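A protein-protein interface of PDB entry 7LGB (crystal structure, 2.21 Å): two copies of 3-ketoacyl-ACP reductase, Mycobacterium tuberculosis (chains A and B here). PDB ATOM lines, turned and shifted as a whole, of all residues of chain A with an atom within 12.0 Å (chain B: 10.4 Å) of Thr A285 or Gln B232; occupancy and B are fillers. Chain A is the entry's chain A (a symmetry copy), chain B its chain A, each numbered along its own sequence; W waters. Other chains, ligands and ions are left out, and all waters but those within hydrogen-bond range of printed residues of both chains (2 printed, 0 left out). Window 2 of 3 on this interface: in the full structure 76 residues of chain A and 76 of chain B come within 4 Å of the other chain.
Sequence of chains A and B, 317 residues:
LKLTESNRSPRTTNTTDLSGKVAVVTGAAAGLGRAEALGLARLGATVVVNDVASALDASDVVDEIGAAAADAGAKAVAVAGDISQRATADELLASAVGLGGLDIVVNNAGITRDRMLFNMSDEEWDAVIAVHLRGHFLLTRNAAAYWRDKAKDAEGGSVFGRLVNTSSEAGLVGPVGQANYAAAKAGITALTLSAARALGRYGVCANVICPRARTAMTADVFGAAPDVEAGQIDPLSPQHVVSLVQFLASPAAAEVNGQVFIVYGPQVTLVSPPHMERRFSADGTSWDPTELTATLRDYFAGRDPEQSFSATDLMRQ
CA of Gln B267 touches O of Phe A280, at 3.3 Å. CA of Ser A281 touches O of Pro B266, 3.4 Å away. Ser A281 touches Gln B267. CB of Gln B232 touches CG2 of Thr A285 (3.9 Å). Thr A285 touches Ile B233 (O to CG2, 3.4 Å). CE1 of His B240 touches O of Thr A285 (3.2 Å). CA of Ser A286 touches CB of Pro B266, 3.9 Å away. NE1 of Trp A287 touches O of Pro B266, at 3.8 Å. Trp A287 touches Gln B267. CG of Pro A289 touches OG of Ser B243, 3.9 Å away.
Water W1 bridges OG of Ser B243 and O of Trp A287. Water W2 lies within hydrogen-bond range of a ring nitrogen (ND1) of His B240 and the backbone NH (N) of Trp A287.
Of the 12 printed residues of chain A, 9 touch a printed residue of chain B. Along chain A the printed residues that touch a printed residue of chain B span positions 280 to 292. Among the printed residues, no Asp or Glu carboxylate lies within 4 Å of a Lys or Arg side-chain nitrogen of the other chain.
No position is printed for both chains.
The backbone carbonyl oxygen (O) of Val B268 sits at hydrogen-bond distance from the backbone NH (N) of Phe A280, at 2.6 Å. The backbone NH of Ala A282 is in hydrogen-bond range of the backbone carbonyl oxygen of Pro B266, 2.9 Å away.
NE2 of His B240 is in hydrogen-bond range of O of Asp B234. O of Gln B239 is in hydrogen-bond range of OG of Ser B243. O of Tyr B264 sits at hydrogen-bond distance from NE2 of Gln B267 (3.1 Å). A ring nitrogen (ND1) of His B240 sits close to the backbone carbonyl oxygen (O) of Gly B265 (3.3 Å). The backbone carbonyl oxygen (O) of Phe A280 is in hydrogen-bond range of the indole nitrogen (NE1) of Trp A287.
Thr A285 touches just these residues of chain B: Gln B232 (3.9 Å), Ile B233 (3.4 Å), His B240 (3.2 Å) and Pro B266 (3.6 Å). Of chain A, only Thr A285 comes within 4 Å of Gln B232. Of chain B, only Pro B266 comes within 4 Å of Gly A284. Printed residues of chain B within 4 Å of Ser A286: Pro B266 (3.9 Å). No residue of chain A comes within 4 Å of Pro B235. No residue of chain A comes within 4 Å of Gly B265. Of chain A, only Ser A281 (3.4 Å), Ala A282 (2.9 Å), Gly A284 (3.5 Å), Thr A285 (3.6 Å), Ser A286 (3.9 Å) and Trp A287 (3.8 Å) come within 4 Å of Pro B266. Of the printed residues of chain A, His B240 touches Thr A285. Of the printed residues of chain B, Phe A280 touches Gln B267 and Val B268. Printed residues of chain B within 4 Å of Ala A282: Pro B266. The nearest residue of chain B that does not touch Thr A285 is Gly B265 (5.2 Å). The nearest printed residue of chain A that does not touch Val B268 is Trp A287 (4.2 Å).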
ATOM      1  N   PHE A 280      -3.823 -31.237   4.420  1.00  0.00           N
ATOM      2  CA  PHE A 280      -3.972 -31.309   2.968  1.00  0.00           C
ATOM      3  C   PHE A 280      -2.627 -30.959   2.331  1.00  0.00           C
ATOM      4  O   PHE A 280      -2.293 -29.780   2.166  1.00  0.00           O
ATOM      5  CB  PHE A 280      -5.081 -30.381   2.487  1.00  0.00           C
ATOM      6  CG  PHE A 280      -6.413 -30.619   3.143  1.00  0.00           C
ATOM      7  CD1 PHE A 280      -7.319 -31.522   2.600  1.00  0.00           C
ATOM      8  CD2 PHE A 280      -6.779 -29.912   4.279  1.00  0.00           C
ATOM      9  CE1 PHE A 280      -8.559 -31.721   3.187  1.00  0.00           C
ATOM     10  CE2 PHE A 280      -8.011 -30.108   4.871  1.00  0.00           C
ATOM     11  CZ  PHE A 280      -8.904 -31.009   4.326  1.00  0.00           C
ATOM     12  N   SER A 281      -1.869 -31.980   1.953  1.00  0.00           N
ATOM     13  CA  SER A 281      -0.528 -31.822   1.406  1.00  0.00           C
ATOM     14  C   SER A 281      -0.519 -32.037  -0.099  1.00  0.00           C
ATOM     15  O   SER A 281      -1.139 -32.976  -0.607  1.00  0.00           O
ATOM     16  CB  SER A 281       0.448 -32.813   2.054  1.00  0.00           C
ATOM     17  OG  SER A 281       0.498 -32.624   3.453  1.00  0.00           O
ATOM     18  N   ALA A 282       0.187 -31.157  -0.805  1.00  0.00           N
ATOM     19  CA  ALA A 282       0.550 -31.420  -2.184  1.00  0.00           C
ATOM     20  C   ALA A 282       1.634 -32.493  -2.234  1.00  0.00           C
ATOM     21  O   ALA A 282       2.366 -32.722  -1.266  1.00  0.00           O
ATOM     22  CB  ALA A 282       1.043 -30.146  -2.866  1.00  0.00           C
ATOM     23  N   ASP A 283       1.729 -33.160  -3.372  1.00  0.00           N
ATOM     24  CA  ASP A 283       2.720 -34.217  -3.511  1.00  0.00           C
ATOM     25  C   ASP A 283       4.100 -33.699  -3.899  1.00  0.00           C
ATOM     26  O   ASP A 283       5.074 -34.453  -3.792  1.00  0.00           O
ATOM     27  CB  ASP A 283       2.233 -35.247  -4.530  1.00  0.00           C
ATOM     28  CG  ASP A 283       1.002 -35.985  -4.050  1.00  0.00           C
ATOM     29  OD1 ASP A 283       0.734 -35.947  -2.832  1.00  0.00           O
ATOM     30  OD2 ASP A 283       0.309 -36.608  -4.873  1.00  0.00           O
ATOM     31  N   GLY A 284       4.210 -32.440  -4.319  1.00  0.00           N
ATOM     32  CA  GLY A 284       5.490 -31.860  -4.680  1.00  0.00           C
ATOM     33  C   GLY A 284       5.850 -30.649  -3.846  1.00  0.00           C
ATOM     34  O   GLY A 284       5.409 -30.524  -2.699  1.00  0.00           O
ATOM     35  N   THR A 285       6.638 -29.737  -4.415  1.00  0.00           N
ATOM     36  CA  THR A 285       7.160 -28.610  -3.652  1.00  0.00           C
ATOM     37  C   THR A 285       6.138 -27.506  -3.434  1.00  0.00           C
ATOM     38  O   THR A 285       6.358 -26.660  -2.562  1.00  0.00           O
ATOM     39  CB  THR A 285       8.404 -28.028  -4.336  1.00  0.00           C
ATOM     40  OG1 THR A 285       8.068 -27.583  -5.661  1.00  0.00           O
ATOM     41  CG2 THR A 285       9.494 -29.081  -4.416  1.00  0.00           C
ATOM     42  N   SER A 286       5.034 -27.490  -4.182  1.00  0.00           N
ATOM     43  CA  SER A 286       3.992 -26.491  -3.971  1.00  0.00           C
ATOM     44  C   SER A 286       2.637 -27.048  -4.391  1.00  0.00           C
ATOM     45  O   SER A 286       2.547 -27.917  -5.269  1.00  0.00           O
ATOM     46  CB  SER A 286       4.268 -25.191  -4.750  1.00  0.00           C
ATOM     47  OG  SER A 286       4.168 -25.397  -6.153  1.00  0.00           O
ATOM     48  N   TRP A 287       1.588 -26.540  -3.737  1.00  0.00           N
ATOM     49  CA  TRP A 287       0.217 -26.773  -4.175  1.00  0.00           C
ATOM     50  C   TRP A 287      -0.027 -26.070  -5.504  1.00  0.00           C
ATOM     51  O   TRP A 287       0.249 -24.876  -5.644  1.00  0.00           O
ATOM     52  CB  TRP A 287      -0.782 -26.242  -3.137  1.00  0.00           C
ATOM     53  CG  TRP A 287      -1.331 -27.252  -2.165  1.00  0.00           C
ATOM     54  CD1 TRP A 287      -1.162 -27.261  -0.800  1.00  0.00           C
ATOM     55  CD2 TRP A 287      -2.148 -28.386  -2.473  1.00  0.00           C
ATOM     56  NE1 TRP A 287      -1.818 -28.341  -0.247  1.00  0.00           N
ATOM     57  CE2 TRP A 287      -2.434 -29.043  -1.254  1.00  0.00           C
ATOM     58  CE3 TRP A 287      -2.667 -28.911  -3.663  1.00  0.00           C
ATOM     59  CZ2 TRP A 287      -3.212 -30.201  -1.194  1.00  0.00           C
ATOM     60  CZ3 TRP A 287      -3.439 -30.068  -3.604  1.00  0.00           C
ATOM     61  CH2 TRP A 287      -3.706 -30.697  -2.374  1.00  0.00           C
ATOM     62  N   ASP A 288      -0.566 -26.789  -6.474  1.00  0.00           N
ATOM     63  CA  ASP A 288      -1.190 -26.095  -7.593  1.00  0.00           C
ATOM     64  C   ASP A 288      -2.473 -25.443  -7.092  1.00  0.00           C
ATOM     65  O   ASP A 288      -3.305 -26.122  -6.486  1.00  0.00           O
ATOM     66  CB  ASP A 288      -1.499 -27.031  -8.746  1.00  0.00           C
ATOM     67  CG  ASP A 288      -2.189 -26.315  -9.875  1.00  0.00           C
ATOM     68  OD1 ASP A 288      -1.483 -25.769 -10.740  1.00  0.00           O
ATOM     69  OD2 ASP A 288      -3.432 -26.253  -9.871  1.00  0.00           O
ATOM     70  N   PRO A 289      -2.658 -24.136  -7.292  1.00  0.00           N
ATOM     71  CA  PRO A 289      -3.804 -23.468  -6.650  1.00  0.00           C
ATOM     72  C   PRO A 289      -5.157 -24.018  -7.080  1.00  0.00           C
ATOM     73  O   PRO A 289      -6.035 -24.190  -6.233  1.00  0.00           O
ATOM     74  CB  PRO A 289      -3.622 -21.996  -7.051  1.00  0.00           C
ATOM     75  CG  PRO A 289      -2.167 -21.873  -7.430  1.00  0.00           C
ATOM     76  CD  PRO A 289      -1.793 -23.193  -8.020  1.00  0.00           C
ATOM     77  N   GLU A 291      -5.718 -27.008  -7.956  1.00  0.00           N
ATOM     78  CA  GLU A 291      -5.789 -28.324  -7.329  1.00  0.00           C
ATOM     79  C   GLU A 291      -6.107 -28.214  -5.843  1.00  0.00           C
ATOM     80  O   GLU A 291      -6.907 -28.997  -5.314  1.00  0.00           O
ATOM     81  CB  GLU A 291      -4.473 -29.066  -7.532  1.00  0.00           C
ATOM     82  CG  GLU A 291      -4.589 -30.554  -7.363  1.00  0.00           C
ATOM     83  CD  GLU A 291      -5.059 -31.220  -8.628  1.00  0.00           C
ATOM     84  OE1 GLU A 291      -4.672 -30.748  -9.718  1.00  0.00           O
ATOM     85  OE2 GLU A 291      -5.822 -32.206  -8.536  1.00  0.00           O
ATOM     86  N   LEU A 292      -5.472 -27.271  -5.146  1.00  0.00           N
ATOM     87  CA  LEU A 292      -5.821 -27.047  -3.749  1.00  0.00           C
ATOM     88  C   LEU A 292      -7.299 -26.706  -3.616  1.00  0.00           C
ATOM     89  O   LEU A 292      -7.997 -27.239  -2.743  1.00  0.00           O
ATOM     90  CB  LEU A 292      -4.955 -25.932  -3.167  1.00  0.00           C
ATOM     91  CG  LEU A 292      -5.332 -25.468  -1.764  1.00  0.00           C
ATOM     92  CD1 LEU A 292      -5.177 -26.621  -0.772  1.00  0.00           C
ATOM     93  CD2 LEU A 292      -4.484 -24.243  -1.342  1.00  0.00           C
ATOM     94  N   ALA B 225      16.089 -17.248   2.412  1.00  0.00           N
ATOM     95  CA  ALA B 225      15.664 -18.228   1.418  1.00  0.00           C
ATOM     96  C   ALA B 225      16.873 -18.970   0.863  1.00  0.00           C
ATOM     97  O   ALA B 225      17.826 -18.333   0.407  1.00  0.00           O
ATOM     98  CB  ALA B 225      14.909 -17.540   0.287  1.00  0.00           C
ATOM     99  N   PRO B 226      16.868 -20.312   0.868  1.00  0.00           N
ATOM    100  CA  PRO B 226      17.949 -21.163   0.351  1.00  0.00           C
ATOM    101  C   PRO B 226      18.404 -20.785  -1.060  1.00  0.00           C
ATOM    102  O   PRO B 226      17.615 -20.219  -1.819  1.00  0.00           O
ATOM    103  CB  PRO B 226      17.323 -22.561   0.348  1.00  0.00           C
ATOM    104  CG  PRO B 226      16.263 -22.506   1.388  1.00  0.00           C
ATOM    105  CD  PRO B 226      15.731 -21.101   1.374  1.00  0.00           C
ATOM    106  N   GLN B 232      13.718 -25.249  -7.188  1.00  0.00           N
ATOM    107  CA  GLN B 232      12.289 -25.434  -6.959  1.00  0.00           C
ATOM    108  C   GLN B 232      11.663 -24.161  -6.402  1.00  0.00           C
ATOM    109  O   GLN B 232      11.709 -23.106  -7.030  1.00  0.00           O
ATOM    110  CB  GLN B 232      12.045 -26.607  -6.011  1.00  0.00           C
ATOM    111  N   ILE B 233      11.071 -24.267  -5.216  1.00  0.00           N
ATOM    112  CA  ILE B 233      10.463 -23.128  -4.545  1.00  0.00           C
ATOM    113  C   ILE B 233      10.872 -23.162  -3.076  1.00  0.00           C
ATOM    114  O   ILE B 233      11.089 -24.229  -2.495  1.00  0.00           O
ATOM    115  CB  ILE B 233       8.925 -23.126  -4.716  1.00  0.00           C
ATOM    116  CG1 ILE B 233       8.314 -21.842  -4.154  1.00  0.00           C
ATOM    117  CG2 ILE B 233       8.313 -24.360  -4.077  1.00  0.00           C
ATOM    118  CD1 ILE B 233       6.791 -21.860  -4.061  1.00  0.00           C
ATOM    119  N   ASP B 234      11.025 -21.980  -2.494  1.00  0.00           N
ATOM    120  CA  ASP B 234      11.358 -21.845  -1.086  1.00  0.00           C
ATOM    121  C   ASP B 234      10.312 -22.568  -0.237  1.00  0.00           C
ATOM    122  O   ASP B 234       9.110 -22.286  -0.371  1.00  0.00           O
ATOM    123  CB  ASP B 234      11.439 -20.356  -0.739  1.00  0.00           C
ATOM    124  CG  ASP B 234      11.696 -20.087   0.744  1.00  0.00           C
ATOM    125  OD1 ASP B 234      11.923 -21.015   1.547  1.00  0.00           O
ATOM    126  OD2 ASP B 234      11.648 -18.903   1.116  1.00  0.00           O
ATOM    127  N   PRO B 235      10.716 -23.512   0.620  1.00  0.00           N
ATOM    128  CA  PRO B 235       9.741 -24.194   1.490  1.00  0.00           C
ATOM    129  C   PRO B 235       8.903 -23.261   2.337  1.00  0.00           C
ATOM    130  O   PRO B 235       7.812 -23.655   2.754  1.00  0.00           O
ATOM    131  CB  PRO B 235      10.622 -25.094   2.371  1.00  0.00           C
ATOM    132  CG  PRO B 235      11.840 -25.347   1.552  1.00  0.00           C
ATOM    133  CD  PRO B 235      12.060 -24.111   0.706  1.00  0.00           C
ATOM    134  N   LEU B 236       9.369 -22.046   2.628  1.00  0.00           N
ATOM    135  CA  LEU B 236       8.574 -21.080   3.377  1.00  0.00           C
ATOM    136  C   LEU B 236       8.201 -19.864   2.530  1.00  0.00           C
ATOM    137  O   LEU B 236       8.004 -18.773   3.064  1.00  0.00           O
ATOM    138  CB  LEU B 236       9.300 -20.636   4.645  1.00  0.00           C
ATOM    139  CG  LEU B 236       9.377 -21.641   5.809  1.00  0.00           C
ATOM    140  CD1 LEU B 236      10.359 -21.158   6.877  1.00  0.00           C
ATOM    141  CD2 LEU B 236       8.010 -21.890   6.419  1.00  0.00           C
ATOM    142  N   SER B 237       8.089 -20.040   1.219  1.00  0.00           N
ATOM    143  CA  SER B 237       7.635 -18.957   0.357  1.00  0.00           C
ATOM    144  C   SER B 237       6.292 -18.397   0.827  1.00  0.00           C
ATOM    145  O   SER B 237       5.402 -19.166   1.217  1.00  0.00           O
ATOM    146  CB  SER B 237       7.480 -19.446  -1.081  1.00  0.00           C
ATOM    147  OG  SER B 237       7.018 -18.378  -1.877  1.00  0.00           O
ATOM    148  N   PRO B 238       6.097 -17.072   0.772  1.00  0.00           N
ATOM    149  CA  PRO B 238       4.743 -16.510   0.958  1.00  0.00           C
ATOM    150  C   PRO B 238       3.710 -17.102   0.013  1.00  0.00           C
ATOM    151  O   PRO B 238       2.514 -17.096   0.325  1.00  0.00           O
ATOM    152  CB  PRO B 238       4.946 -15.013   0.680  1.00  0.00           C
ATOM    153  CG  PRO B 238       6.373 -14.762   0.940  1.00  0.00           C
ATOM    154  CD  PRO B 238       7.109 -16.023   0.568  1.00  0.00           C
ATOM    155  N   GLN B 239       4.153 -17.618  -1.139  1.00  0.00           N
ATOM    156  CA  GLN B 239       3.234 -18.135  -2.144  1.00  0.00           C
ATOM    157  C   GLN B 239       2.434 -19.318  -1.628  1.00  0.00           C
ATOM    158  O   GLN B 239       1.288 -19.513  -2.049  1.00  0.00           O
ATOM    159  CB  GLN B 239       4.011 -18.535  -3.396  1.00  0.00           C
ATOM    160  CG  GLN B 239       4.332 -17.352  -4.290  1.00  0.00           C
ATOM    161  CD  GLN B 239       3.107 -16.495  -4.578  1.00  0.00           C
ATOM    162  OE1 GLN B 239       2.079 -16.993  -5.049  1.00  0.00           O
ATOM    163  NE2 GLN B 239       3.212 -15.201  -4.288  1.00  0.00           N
ATOM    164  N   HIS B 240       3.034 -20.132  -0.755  1.00  0.00           N
ATOM    165  CA  HIS B 240       2.323 -21.244  -0.133  1.00  0.00           C
ATOM    166  C   HIS B 240       1.085 -20.761   0.601  1.00  0.00           C
ATOM    167  O   HIS B 240       0.054 -21.442   0.606  1.00  0.00           O
ATOM    168  CB  HIS B 240       3.239 -21.975   0.844  1.00  0.00           C
ATOM    169  CG  HIS B 240       4.434 -22.600   0.200  1.00  0.00           C
ATOM    170  ND1 HIS B 240       4.333 -23.626  -0.712  1.00  0.00           N
ATOM    171  CD2 HIS B 240       5.759 -22.359   0.354  1.00  0.00           C
ATOM    172  CE1 HIS B 240       5.544 -23.979  -1.109  1.00  0.00           C
ATOM    173  NE2 HIS B 240       6.427 -23.234  -0.468  1.00  0.00           N
ATOM    174  N   VAL B 241       1.186 -19.600   1.253  1.00  0.00           N
ATOM    175  CA  VAL B 241       0.043 -19.000   1.928  1.00  0.00           C
ATOM    176  C   VAL B 241      -0.911 -18.379   0.917  1.00  0.00           C
ATOM    177  O   VAL B 241      -2.135 -18.509   1.044  1.00  0.00           O
ATOM    178  CB  VAL B 241       0.521 -17.958   2.958  1.00  0.00           C
ATOM    179  CG1 VAL B 241      -0.675 -17.401   3.770  1.00  0.00           C
ATOM    180  CG2 VAL B 241       1.575 -18.560   3.885  1.00  0.00           C
ATOM    181  N   SER B 243      -1.733 -19.166  -2.044  1.00  0.00           N
ATOM    182  CA  SER B 243      -2.612 -20.143  -2.684  1.00  0.00           C
ATOM    183  C   SER B 243      -3.856 -20.408  -1.841  1.00  0.00           C
ATOM    184  O   SER B 243      -4.972 -20.467  -2.373  1.00  0.00           O
ATOM    185  CB  SER B 243      -1.860 -21.445  -2.945  1.00  0.00           C
ATOM    186  OG  SER B 243      -0.821 -21.254  -3.876  1.00  0.00           O
ATOM    187  N   TYR B 264       1.758 -23.477   5.652  1.00  0.00           N
ATOM    188  CA  TYR B 264       3.126 -23.123   5.301  1.00  0.00           C
ATOM    189  C   TYR B 264       3.720 -24.281   4.522  1.00  0.00           C
ATOM    190  O   TYR B 264       3.431 -25.446   4.810  1.00  0.00           O
ATOM    191  CB  TYR B 264       3.987 -22.799   6.531  1.00  0.00           C
ATOM    192  CG  TYR B 264       4.059 -23.880   7.594  1.00  0.00           C
ATOM    193  CD1 TYR B 264       5.007 -24.889   7.521  1.00  0.00           C
ATOM    194  CD2 TYR B 264       3.198 -23.860   8.690  1.00  0.00           C
ATOM    195  CE1 TYR B 264       5.085 -25.865   8.490  1.00  0.00           C
ATOM    196  CE2 TYR B 264       3.265 -24.831   9.674  1.00  0.00           C
ATOM    197  CZ  TYR B 264       4.205 -25.830   9.568  1.00  0.00           C
ATOM    198  OH  TYR B 264       4.274 -26.793  10.542  1.00  0.00           O
ATOM    199  N   GLY B 265       4.535 -23.957   3.529  1.00  0.00           N
ATOM    200  CA  GLY B 265       5.002 -24.958   2.611  1.00  0.00           C
ATOM    201  C   GLY B 265       3.835 -25.561   1.855  1.00  0.00           C
ATOM    202  O   GLY B 265       2.732 -25.006   1.819  1.00  0.00           O
ATOM    203  N   PRO B 266       4.060 -26.726   1.250  1.00  0.00           N
ATOM    204  CA  PRO B 266       3.055 -27.374   0.393  1.00  0.00           C
ATOM    205  C   PRO B 266       1.996 -28.157   1.172  1.00  0.00           C
ATOM    206  O   PRO B 266       1.690 -29.308   0.862  1.00  0.00           O
ATOM    207  CB  PRO B 266       3.914 -28.291  -0.487  1.00  0.00           C
ATOM    208  CG  PRO B 266       5.096 -28.642   0.374  1.00  0.00           C
ATOM    209  CD  PRO B 266       5.330 -27.474   1.302  1.00  0.00           C
ATOM    210  N   GLN B 267       1.438 -27.532   2.205  1.00  0.00           N
ATOM    211  CA  GLN B 267       0.426 -28.181   3.019  1.00  0.00           C
ATOM    212  C   GLN B 267      -0.465 -27.123   3.654  1.00  0.00           C
ATOM    213  O   GLN B 267      -0.022 -26.008   3.947  1.00  0.00           O
ATOM    214  CB  GLN B 267       1.051 -29.062   4.109  1.00  0.00           C
ATOM    215  CG  GLN B 267       1.897 -28.295   5.127  1.00  0.00           C
ATOM    216  CD  GLN B 267       1.097 -27.743   6.289  1.00  0.00           C
ATOM    217  OE1 GLN B 267       0.009 -28.234   6.596  1.00  0.00           O
ATOM    218  NE2 GLN B 267       1.635 -26.706   6.944  1.00  0.00           N
ATOM    219  N   VAL B 268      -1.732 -27.495   3.837  1.00  0.00           N
ATOM    220  CA  VAL B 268      -2.720 -26.741   4.588  1.00  0.00           C
ATOM    221  C   VAL B 268      -3.310 -27.693   5.621  1.00  0.00           C
ATOM    222  O   VAL B 268      -3.651 -28.836   5.286  1.00  0.00           O
ATOM    223  CB  VAL B 268      -3.825 -26.181   3.670  1.00  0.00           C
ATOM    224  CG1 VAL B 268      -4.893 -25.492   4.496  1.00  0.00           C
ATOM    225  CG2 VAL B 268      -3.233 -25.213   2.654  1.00  0.00           C
HETATM  226  O   HOH W   1       1.083 -23.009  -3.858  1.00  0.00           O
HETATM  227  O   HOH W   2       1.751 -24.400  -1.753  1.00  0.00           O
